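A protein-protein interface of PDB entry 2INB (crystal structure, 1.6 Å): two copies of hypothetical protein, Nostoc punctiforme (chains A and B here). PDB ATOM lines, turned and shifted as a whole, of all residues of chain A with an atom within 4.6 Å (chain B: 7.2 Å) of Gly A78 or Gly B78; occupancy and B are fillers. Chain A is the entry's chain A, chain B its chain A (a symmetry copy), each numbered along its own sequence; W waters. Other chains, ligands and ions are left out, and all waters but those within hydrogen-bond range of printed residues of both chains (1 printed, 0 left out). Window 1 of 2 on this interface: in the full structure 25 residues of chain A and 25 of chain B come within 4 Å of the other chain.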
ATOM      1  N   HIS A  74       4.428 -10.979  26.271  1.00  0.00           N
ATOM      2  CA  HIS A  74       4.516 -10.855  24.827  1.00  0.00           C
ATOM      3  C   HIS A  74       4.940 -12.181  24.165  1.00  0.00           C
ATOM      4  O   HIS A  74       4.316 -12.652  23.200  1.00  0.00           O
ATOM      5  CB  HIS A  74       5.559  -9.828  24.389  1.00  0.00           C
ATOM      6  CG  HIS A  74       5.274  -8.432  24.801  1.00  0.00           C
ATOM      7  ND1 HIS A  74       4.041  -7.849  24.652  1.00  0.00           N
ATOM      8  CD2 HIS A  74       6.107  -7.468  25.274  1.00  0.00           C
ATOM      9  CE1 HIS A  74       4.113  -6.589  25.070  1.00  0.00           C
ATOM     10  NE2 HIS A  74       5.356  -6.338  25.464  1.00  0.00           N
ATOM     11  N   THR A  75       6.013 -12.787  24.692  1.00  0.00           N
ATOM     12  CA  THR A  75       6.520 -14.041  24.128  1.00  0.00           C
ATOM     13  C   THR A  75       5.531 -15.160  24.373  1.00  0.00           C
ATOM     14  O   THR A  75       5.275 -15.968  23.482  1.00  0.00           O
ATOM     15  CB  THR A  75       7.892 -14.356  24.739  1.00  0.00           C
ATOM     16  OG1 THR A  75       8.813 -13.313  24.353  1.00  0.00           O
ATOM     17  CG2 THR A  75       8.432 -15.765  24.367  1.00  0.00           C
ATOM     18  N   ALA A  76       4.942 -15.211  25.570  1.00  0.00           N
ATOM     19  CA  ALA A  76       3.983 -16.268  25.875  1.00  0.00           C
ATOM     20  C   ALA A  76       2.779 -16.233  24.943  1.00  0.00           C
ATOM     21  O   ALA A  76       2.255 -17.269  24.518  1.00  0.00           O
ATOM     22  CB  ALA A  76       3.496 -16.208  27.354  1.00  0.00           C
ATOM     23  N   LEU A  77       2.307 -15.029  24.671  1.00  0.00           N
ATOM     24  CA  LEU A  77       1.140 -14.826  23.800  1.00  0.00           C
ATOM     25  C   LEU A  77       1.474 -15.196  22.357  1.00  0.00           C
ATOM     26  O   LEU A  77       0.703 -15.862  21.671  1.00  0.00           O
ATOM     27  CB  LEU A  77       0.677 -13.375  23.897  1.00  0.00           C
ATOM     28  CG  LEU A  77      -0.503 -13.018  23.002  1.00  0.00           C
ATOM     29  CD1 LEU A  77      -1.766 -13.876  23.427  1.00  0.00           C
ATOM     30  CD2 LEU A  77      -0.844 -11.489  23.127  1.00  0.00           C
ATOM     31  N   GLY A  78       2.611 -14.733  21.866  1.00  0.00           N
ATOM     32  CA  GLY A  78       3.008 -15.064  20.469  1.00  0.00           C
ATOM     33  C   GLY A  78       3.167 -16.569  20.296  1.00  0.00           C
ATOM     34  O   GLY A  78       2.713 -17.167  19.292  1.00  0.00           O
ATOM     35  N   GLN A  79       3.866 -17.202  21.245  1.00  0.00           N
ATOM     36  CA  GLN A  79       3.988 -18.647  21.236  1.00  0.00           C
ATOM     37  C   GLN A  79       2.628 -19.308  21.252  1.00  0.00           C
ATOM     38  O   GLN A  79       2.354 -20.289  20.523  1.00  0.00           O
ATOM     39  CB  GLN A  79       4.824 -19.111  22.445  1.00  0.00           C
ATOM     40  CG  GLN A  79       6.302 -18.870  22.266  1.00  0.00           C
ATOM     41  CD  GLN A  79       7.134 -19.183  23.469  1.00  0.00           C
ATOM     42  OE1 GLN A  79       6.624 -19.241  24.580  1.00  0.00           O
ATOM     43  NE2 GLN A  79       8.451 -19.224  23.266  1.00  0.00           N
ATOM     44  N   PHE A  80       1.745 -18.808  22.107  1.00  0.00           N
ATOM     45  CA  PHE A  80       0.415 -19.413  22.212  1.00  0.00           C
ATOM     46  C   PHE A  80      -0.300 -19.393  20.843  1.00  0.00           C
ATOM     47  O   PHE A  80      -0.843 -20.404  20.336  1.00  0.00           O
ATOM     48  CB  PHE A  80      -0.451 -18.722  23.277  1.00  0.00           C
ATOM     49  CG  PHE A  80      -1.789 -19.369  23.423  1.00  0.00           C
ATOM     50  CD1 PHE A  80      -1.992 -20.442  24.310  1.00  0.00           C
ATOM     51  CD2 PHE A  80      -2.892 -18.938  22.691  1.00  0.00           C
ATOM     52  CE1 PHE A  80      -3.217 -21.049  24.419  1.00  0.00           C
ATOM     53  CE2 PHE A  80      -4.134 -19.582  22.811  1.00  0.00           C
ATOM     54  CZ  PHE A  80      -4.294 -20.634  23.672  1.00  0.00           C
ATOM     55  N   ILE A  81      -0.259 -18.225  20.204  1.00  0.00           N
ATOM     56  CA  ILE A  81      -0.966 -18.045  18.925  1.00  0.00           C
ATOM     57  C   ILE A  81      -0.369 -18.976  17.863  1.00  0.00           C
ATOM     58  O   ILE A  81      -1.081 -19.640  17.058  1.00  0.00           O
ATOM     59  CB  ILE A  81      -0.961 -16.544  18.529  1.00  0.00           C
ATOM     60  CG1 ILE A  81      -1.923 -15.792  19.463  1.00  0.00           C
ATOM     61  CG2 ILE A  81      -1.370 -16.324  17.034  1.00  0.00           C
ATOM     62  CD1 ILE A  81      -1.782 -14.310  19.413  1.00  0.00           C
ATOM     63  N   ASN A  82       0.966 -19.000  17.819  1.00  0.00           N
ATOM     64  CA  ASN A  82       1.617 -19.810  16.790  1.00  0.00           C
ATOM     65  C   ASN A  82       1.450 -21.305  17.042  1.00  0.00           C
ATOM     66  O   ASN A  82       1.162 -22.059  16.086  1.00  0.00           O
ATOM     67  CB  ASN A  82       3.078 -19.417  16.675  1.00  0.00           C
ATOM     68  CG  ASN A  82       3.283 -18.127  15.930  1.00  0.00           C
ATOM     69  OD1 ASN A  82       2.490 -17.762  15.069  1.00  0.00           O
ATOM     70  ND2 ASN A  82       4.398 -17.442  16.237  1.00  0.00           N
ATOM     71  N   GLU B  59       7.294  -1.274  14.870  1.00  0.00           N
ATOM     72  CA  GLU B  59       8.000  -2.267  15.698  1.00  0.00           C
ATOM     73  C   GLU B  59       9.147  -2.806  14.871  1.00  0.00           C
ATOM     74  O   GLU B  59       8.909  -3.519  13.885  1.00  0.00           O
ATOM     75  CB  GLU B  59       6.988  -3.389  16.049  1.00  0.00           C
ATOM     76  CG  GLU B  59       7.615  -4.593  16.661  1.00  0.00           C
ATOM     77  CD  GLU B  59       6.651  -5.747  16.858  1.00  0.00           C
ATOM     78  OE1 GLU B  59       5.429  -5.526  16.703  1.00  0.00           O
ATOM     79  OE2 GLU B  59       7.171  -6.886  17.142  1.00  0.00           O
ATOM     80  N   GLU B  72      12.298 -15.713  17.276  1.00  0.00           N
ATOM     81  CA  GLU B  72      12.087 -14.276  17.257  1.00  0.00           C
ATOM     82  C   GLU B  72      10.667 -13.992  16.821  1.00  0.00           C
ATOM     83  O   GLU B  72      10.024 -13.085  17.375  1.00  0.00           O
ATOM     84  CB  GLU B  72      13.080 -13.508  16.370  1.00  0.00           C
ATOM     85  CG  GLU B  72      12.816 -12.023  16.323  1.00  0.00           C
ATOM     86  CD  GLU B  72      12.637 -11.404  17.711  1.00  0.00           C
ATOM     87  OE1 GLU B  72      13.344 -11.825  18.659  1.00  0.00           O
ATOM     88  OE2 GLU B  72      11.795 -10.511  17.866  1.00  0.00           O
ATOM     89  N   PHE B  73      10.156 -14.769  15.857  1.00  0.00           N
ATOM     90  CA  PHE B  73       8.814 -14.505  15.330  1.00  0.00           C
ATOM     91  C   PHE B  73       7.779 -14.608  16.454  1.00  0.00           C
ATOM     92  O   PHE B  73       6.834 -13.822  16.504  1.00  0.00           O
ATOM     93  CB  PHE B  73       8.463 -15.422  14.170  1.00  0.00           C
ATOM     94  CG  PHE B  73       7.103 -15.161  13.588  1.00  0.00           C
ATOM     95  CD1 PHE B  73       6.745 -13.911  13.112  1.00  0.00           C
ATOM     96  CD2 PHE B  73       6.193 -16.208  13.490  1.00  0.00           C
ATOM     97  CE1 PHE B  73       5.455 -13.729  12.569  1.00  0.00           C
ATOM     98  CE2 PHE B  73       4.909 -16.011  12.943  1.00  0.00           C
ATOM     99  CZ  PHE B  73       4.582 -14.785  12.461  1.00  0.00           C
ATOM    100  N   HIS B  74       7.924 -15.570  17.346  1.00  0.00           N
ATOM    101  CA  HIS B  74       6.967 -15.664  18.434  1.00  0.00           C
ATOM    102  C   HIS B  74       6.884 -14.350  19.235  1.00  0.00           C
ATOM    103  O   HIS B  74       5.792 -13.819  19.497  1.00  0.00           O
ATOM    104  CB  HIS B  74       7.340 -16.740  19.452  1.00  0.00           C
ATOM    105  CG  HIS B  74       7.343 -18.126  18.925  1.00  0.00           C
ATOM    106  ND1 HIS B  74       6.328 -18.631  18.152  1.00  0.00           N
ATOM    107  CD2 HIS B  74       8.210 -19.150  19.148  1.00  0.00           C
ATOM    108  CE1 HIS B  74       6.597 -19.903  17.874  1.00  0.00           C
ATOM    109  NE2 HIS B  74       7.742 -20.237  18.458  1.00  0.00           N
ATOM    110  N   THR B  75       8.052 -13.822  19.627  1.00  0.00           N
ATOM    111  CA  THR B  75       8.092 -12.587  20.415  1.00  0.00           C
ATOM    112  C   THR B  75       7.628 -11.417  19.574  1.00  0.00           C
ATOM    113  O   THR B  75       6.870 -10.574  20.050  1.00  0.00           O
ATOM    114  CB  THR B  75       9.514 -12.369  20.948  1.00  0.00           C
ATOM    115  OG1 THR B  75       9.836 -13.456  21.843  1.00  0.00           O
ATOM    116  CG2 THR B  75       9.722 -10.987  21.627  1.00  0.00           C
ATOM    117  N   ALA B  76       8.052 -11.361  18.309  1.00  0.00           N
ATOM    118  CA  ALA B  76       7.646 -10.256  17.445  1.00  0.00           C
ATOM    119  C   ALA B  76       6.135 -10.196  17.266  1.00  0.00           C
ATOM    120  O   ALA B  76       5.527  -9.121  17.226  1.00  0.00           O
ATOM    121  CB  ALA B  76       8.333 -10.323  16.049  1.00  0.00           C
ATOM    122  N   LEU B  77       5.538 -11.364  17.099  1.00  0.00           N
ATOM    123  CA  LEU B  77       4.085 -11.474  16.896  1.00  0.00           C
ATOM    124  C   LEU B  77       3.334 -11.090  18.168  1.00  0.00           C
ATOM    125  O   LEU B  77       2.345 -10.362  18.133  1.00  0.00           O
ATOM    126  CB  LEU B  77       3.738 -12.897  16.467  1.00  0.00           C
ATOM    127  CG  LEU B  77       2.251 -13.162  16.270  1.00  0.00           C
ATOM    128  CD1 LEU B  77       1.703 -12.240  15.102  1.00  0.00           C
ATOM    129  CD2 LEU B  77       2.004 -14.670  15.904  1.00  0.00           C
ATOM    130  N   GLY B  78       3.770 -11.608  19.304  1.00  0.00           N
ATOM    131  CA  GLY B  78       3.092 -11.267  20.586  1.00  0.00           C
ATOM    132  C   GLY B  78       3.174  -9.771  20.857  1.00  0.00           C
ATOM    133  O   GLY B  78       2.183  -9.122  21.270  1.00  0.00           O
ATOM    134  N   GLN B  79       4.373  -9.204  20.687  1.00  0.00           N
ATOM    135  CA  GLN B  79       4.540  -7.769  20.814  1.00  0.00           C
ATOM    136  C   GLN B  79       3.625  -7.029  19.865  1.00  0.00           C
ATOM    137  O   GLN B  79       2.978  -6.015  20.218  1.00  0.00           O
ATOM    138  CB  GLN B  79       6.010  -7.385  20.550  1.00  0.00           C
ATOM    139  CG  GLN B  79       6.920  -7.709  21.708  1.00  0.00           C
ATOM    140  CD  GLN B  79       8.373  -7.476  21.441  1.00  0.00           C
ATOM    141  OE1 GLN B  79       8.793  -7.416  20.292  1.00  0.00           O
ATOM    142  NE2 GLN B  79       9.170  -7.509  22.510  1.00  0.00           N
ATOM    143  N   PHE B  80       3.566  -7.495  18.625  1.00  0.00           N
ATOM    144  CA  PHE B  80       2.732  -6.815  17.633  1.00  0.00           C
ATOM    145  C   PHE B  80       1.262  -6.759  18.106  1.00  0.00           C
ATOM    146  O   PHE B  80       0.582  -5.705  18.112  1.00  0.00           O
ATOM    147  CB  PHE B  80       2.821  -7.479  16.250  1.00  0.00           C
ATOM    148  CG  PHE B  80       2.011  -6.757  15.223  1.00  0.00           C
ATOM    149  CD1 PHE B  80       2.552  -5.696  14.476  1.00  0.00           C
ATOM    150  CD2 PHE B  80       0.688  -7.103  14.962  1.00  0.00           C
ATOM    151  CE1 PHE B  80       1.794  -5.019  13.554  1.00  0.00           C
ATOM    152  CE2 PHE B  80      -0.072  -6.390  14.021  1.00  0.00           C
ATOM    153  CZ  PHE B  80       0.481  -5.352  13.320  1.00  0.00           C
ATOM    154  N   ILE B  81       0.773  -7.911  18.562  1.00  0.00           N
ATOM    155  CA  ILE B  81      -0.636  -8.017  18.974  1.00  0.00           C
ATOM    156  C   ILE B  81      -0.901  -7.098  20.172  1.00  0.00           C
ATOM    157  O   ILE B  81      -1.931  -6.373  20.263  1.00  0.00           O
ATOM    158  CB  ILE B  81      -1.000  -9.506  19.223  1.00  0.00           C
ATOM    159  CG1 ILE B  81      -1.074 -10.222  17.864  1.00  0.00           C
ATOM    160  CG2 ILE B  81      -2.352  -9.664  19.996  1.00  0.00           C
ATOM    161  CD1 ILE B  81      -1.096 -11.708  17.963  1.00  0.00           C
ATOM    162  N   ASN B  82       0.019  -7.153  21.140  1.00  0.00           N
ATOM    163  CA  ASN B  82      -0.191  -6.358  22.350  1.00  0.00           C
ATOM    164  C   ASN B  82      -0.044  -4.862  22.090  1.00  0.00           C
ATOM    165  O   ASN B  82      -0.874  -4.069  22.587  1.00  0.00           O
ATOM    166  CB  ASN B  82       0.743  -6.834  23.446  1.00  0.00           C
ATOM    167  CG  ASN B  82       0.289  -8.116  24.089  1.00  0.00           C
ATOM    168  OD1 ASN B  82      -0.900  -8.412  24.138  1.00  0.00           O
ATOM    169  ND2 ASN B  82       1.255  -8.873  24.635  1.00  0.00           N
ATOM    170  N   TYR B  83       0.983  -4.468  21.320  1.00  0.00           N
ATOM    171  CA  TYR B  83       1.122  -3.057  21.020  1.00  0.00           C
ATOM    172  C   TYR B  83      -0.085  -2.564  20.213  1.00  0.00           C
ATOM    173  O   TYR B  83      -0.538  -1.443  20.404  1.00  0.00           O
ATOM    174  CB  TYR B  83       2.431  -2.760  20.269  1.00  0.00           C
ATOM    175  CG  TYR B  83       3.711  -3.055  21.028  1.00  0.00           C
ATOM    176  CD1 TYR B  83       3.791  -2.903  22.395  1.00  0.00           C
ATOM    177  CD2 TYR B  83       4.866  -3.422  20.319  1.00  0.00           C
ATOM    178  CE1 TYR B  83       4.983  -3.179  23.092  1.00  0.00           C
ATOM    179  CE2 TYR B  83       6.066  -3.703  21.007  1.00  0.00           C
ATOM    180  CZ  TYR B  83       6.106  -3.551  22.381  1.00  0.00           C
ATOM    181  OH  TYR B  83       7.284  -3.812  23.077  1.00  0.00           O
ATOM    182  N   ARG B  84      -0.565  -3.377  19.284  1.00  0.00           N
ATOM    183  CA  ARG B  84      -1.690  -2.983  18.442  1.00  0.00           C
ATOM    184  C   ARG B  84      -2.910  -2.760  19.343  1.00  0.00           C
ATOM    185  O   ARG B  84      -3.640  -1.766  19.204  1.00  0.00           O
ATOM    186  CB  ARG B  84      -1.978  -4.049  17.424  1.00  0.00           C
ATOM    187  CG  ARG B  84      -3.156  -3.660  16.557  1.00  0.00           C
ATOM    188  CD  ARG B  84      -3.449  -4.731  15.433  1.00  0.00           C
ATOM    189  NE  ARG B  84      -3.741  -6.032  15.999  1.00  0.00           N
ATOM    190  CZ  ARG B  84      -3.758  -7.153  15.297  1.00  0.00           C
ATOM    191  NH1 ARG B  84      -3.631  -7.102  13.985  1.00  0.00           N
ATOM    192  NH2 ARG B  84      -3.938  -8.300  15.903  1.00  0.00           N
ATOM    193  N   MET B 117       0.450 -17.206   9.464  1.00  0.00           N
ATOM    194  CA  MET B 117       0.245 -16.531  10.757  1.00  0.00           C
ATOM    195  C   MET B 117       0.203 -14.990  10.676  1.00  0.00           C
ATOM    196  O   MET B 117      -0.509 -14.343  11.435  1.00  0.00           O
ATOM    197  CB  MET B 117       1.274 -17.036  11.790  1.00  0.00           C
ATOM    198  CG  MET B 117       1.306 -18.567  11.889  1.00  0.00           C
ATOM    199  SD  MET B 117      -0.463 -19.357  12.203  1.00  0.00           S
ATOM    200  CE  MET B 117      -0.945 -18.279  13.835  1.00  0.00           C
HETATM  201  O   HOH W   1       6.816  -3.955  26.097  1.00  0.00           O
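The side-chain hydroxyl (OG1) of Thr A75 is in hydrogen-bond range of the side-chain hydroxyl (OG1) of Thr B75. The side-chain amide nitrogen (ND2) of Asn B82 is in hydrogen-bond range of a ring nitrogen (ND1) of His A74, at 3.0 Å. The side-chain amide nitrogen (ND2) of Asn A82 sits at hydrogen-bond distance from a ring nitrogen (ND1) of His B74 (3.0 Å).
The backbone carbonyl oxygen (O) of Gly B78 sits close to the side-chain amide nitrogen (ND2) of Asn B82 (3.5 Å). The side-chain amide nitrogen (ND2) of Asn A82 lies close to the backbone carbonyl oxygen (O) of Gly A78 (3.5 Å).
O of His A74 touches CA of Gly B78 (3.2 Å). CG of His A74 touches CG of Gln B79 (3.6 Å). His A74 touches Tyr B83 (NE2 to CE1, 3.97 Å). Leu A77 touches Ile B81 (CD2 to CG2, 3.9 Å). OD1 of Asn B82 touches CD2 of Leu A77, 3.2 Å away. Gly A78 touches His B74 (CA to O, 3.2 Å). Gly B78 touches Gly A78. Gln A79 touches His B74. Ile A81 touches Met B117 (O to CE, 3.5 Å). Met B117 touches Asn A82.
Printed residues of chain B within 4 Å of His A74: Gly B78, Gln B79, Asn B82 and Tyr B83. Of chain B, only His B74 and Gly B78 come within 4 Å of Gly A78. Printed residues of chain B within 4 Å of Ile A81: Leu B77, Ile B81 and Met B117. Glu B72 touches none of the printed residues of chain A. Of the printed residues of chain A, Tyr B83 touches His A74. Arg B84 touches none of the printed residues of chain A. The nearest residue of chain B that does not touch Gly A78 is Leu B77 (4.3 Å). The nearest printed residue of chain A that does not touch Thr B75 is His A74 (4.6 Å).
Hydrophobic or aromatic side chains of chain B that line the printed part of chain A: Phe B73, His B74, Leu B77, Ile B81, Tyr B83 and Met B117. Printed residues of chain A that touch a printed residue of chain B: His A74, Thr A75, Leu A77, Gly A78, Gln A79, Ile A81 and Asn A82. Among the printed residues, 17 pairs touch across the chains.
His A74 touches Gln B79, and with the chains exchanged Gln A79 touches His B74. His A74 touches Asn B82, and with the chains exchanged Asn A82 touches His B74. Leu A77 touches Asn B82, and with the chains exchanged Asn A82 touches Leu B77. Gly A78 touches its own counterpart, Gly B78. Positions printed for both chains: 74, 75, 76, 77, 78, 79, 80, 81 and 82. Of the 17 pairs that touch across the chains among the printed residues, 13 have their exchanged pair printed and touching as well.
Water W1 lies within hydrogen-bond range of NE2 of His A74 (2.9 Å) and OH of Tyr B83 (3.1 Å).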
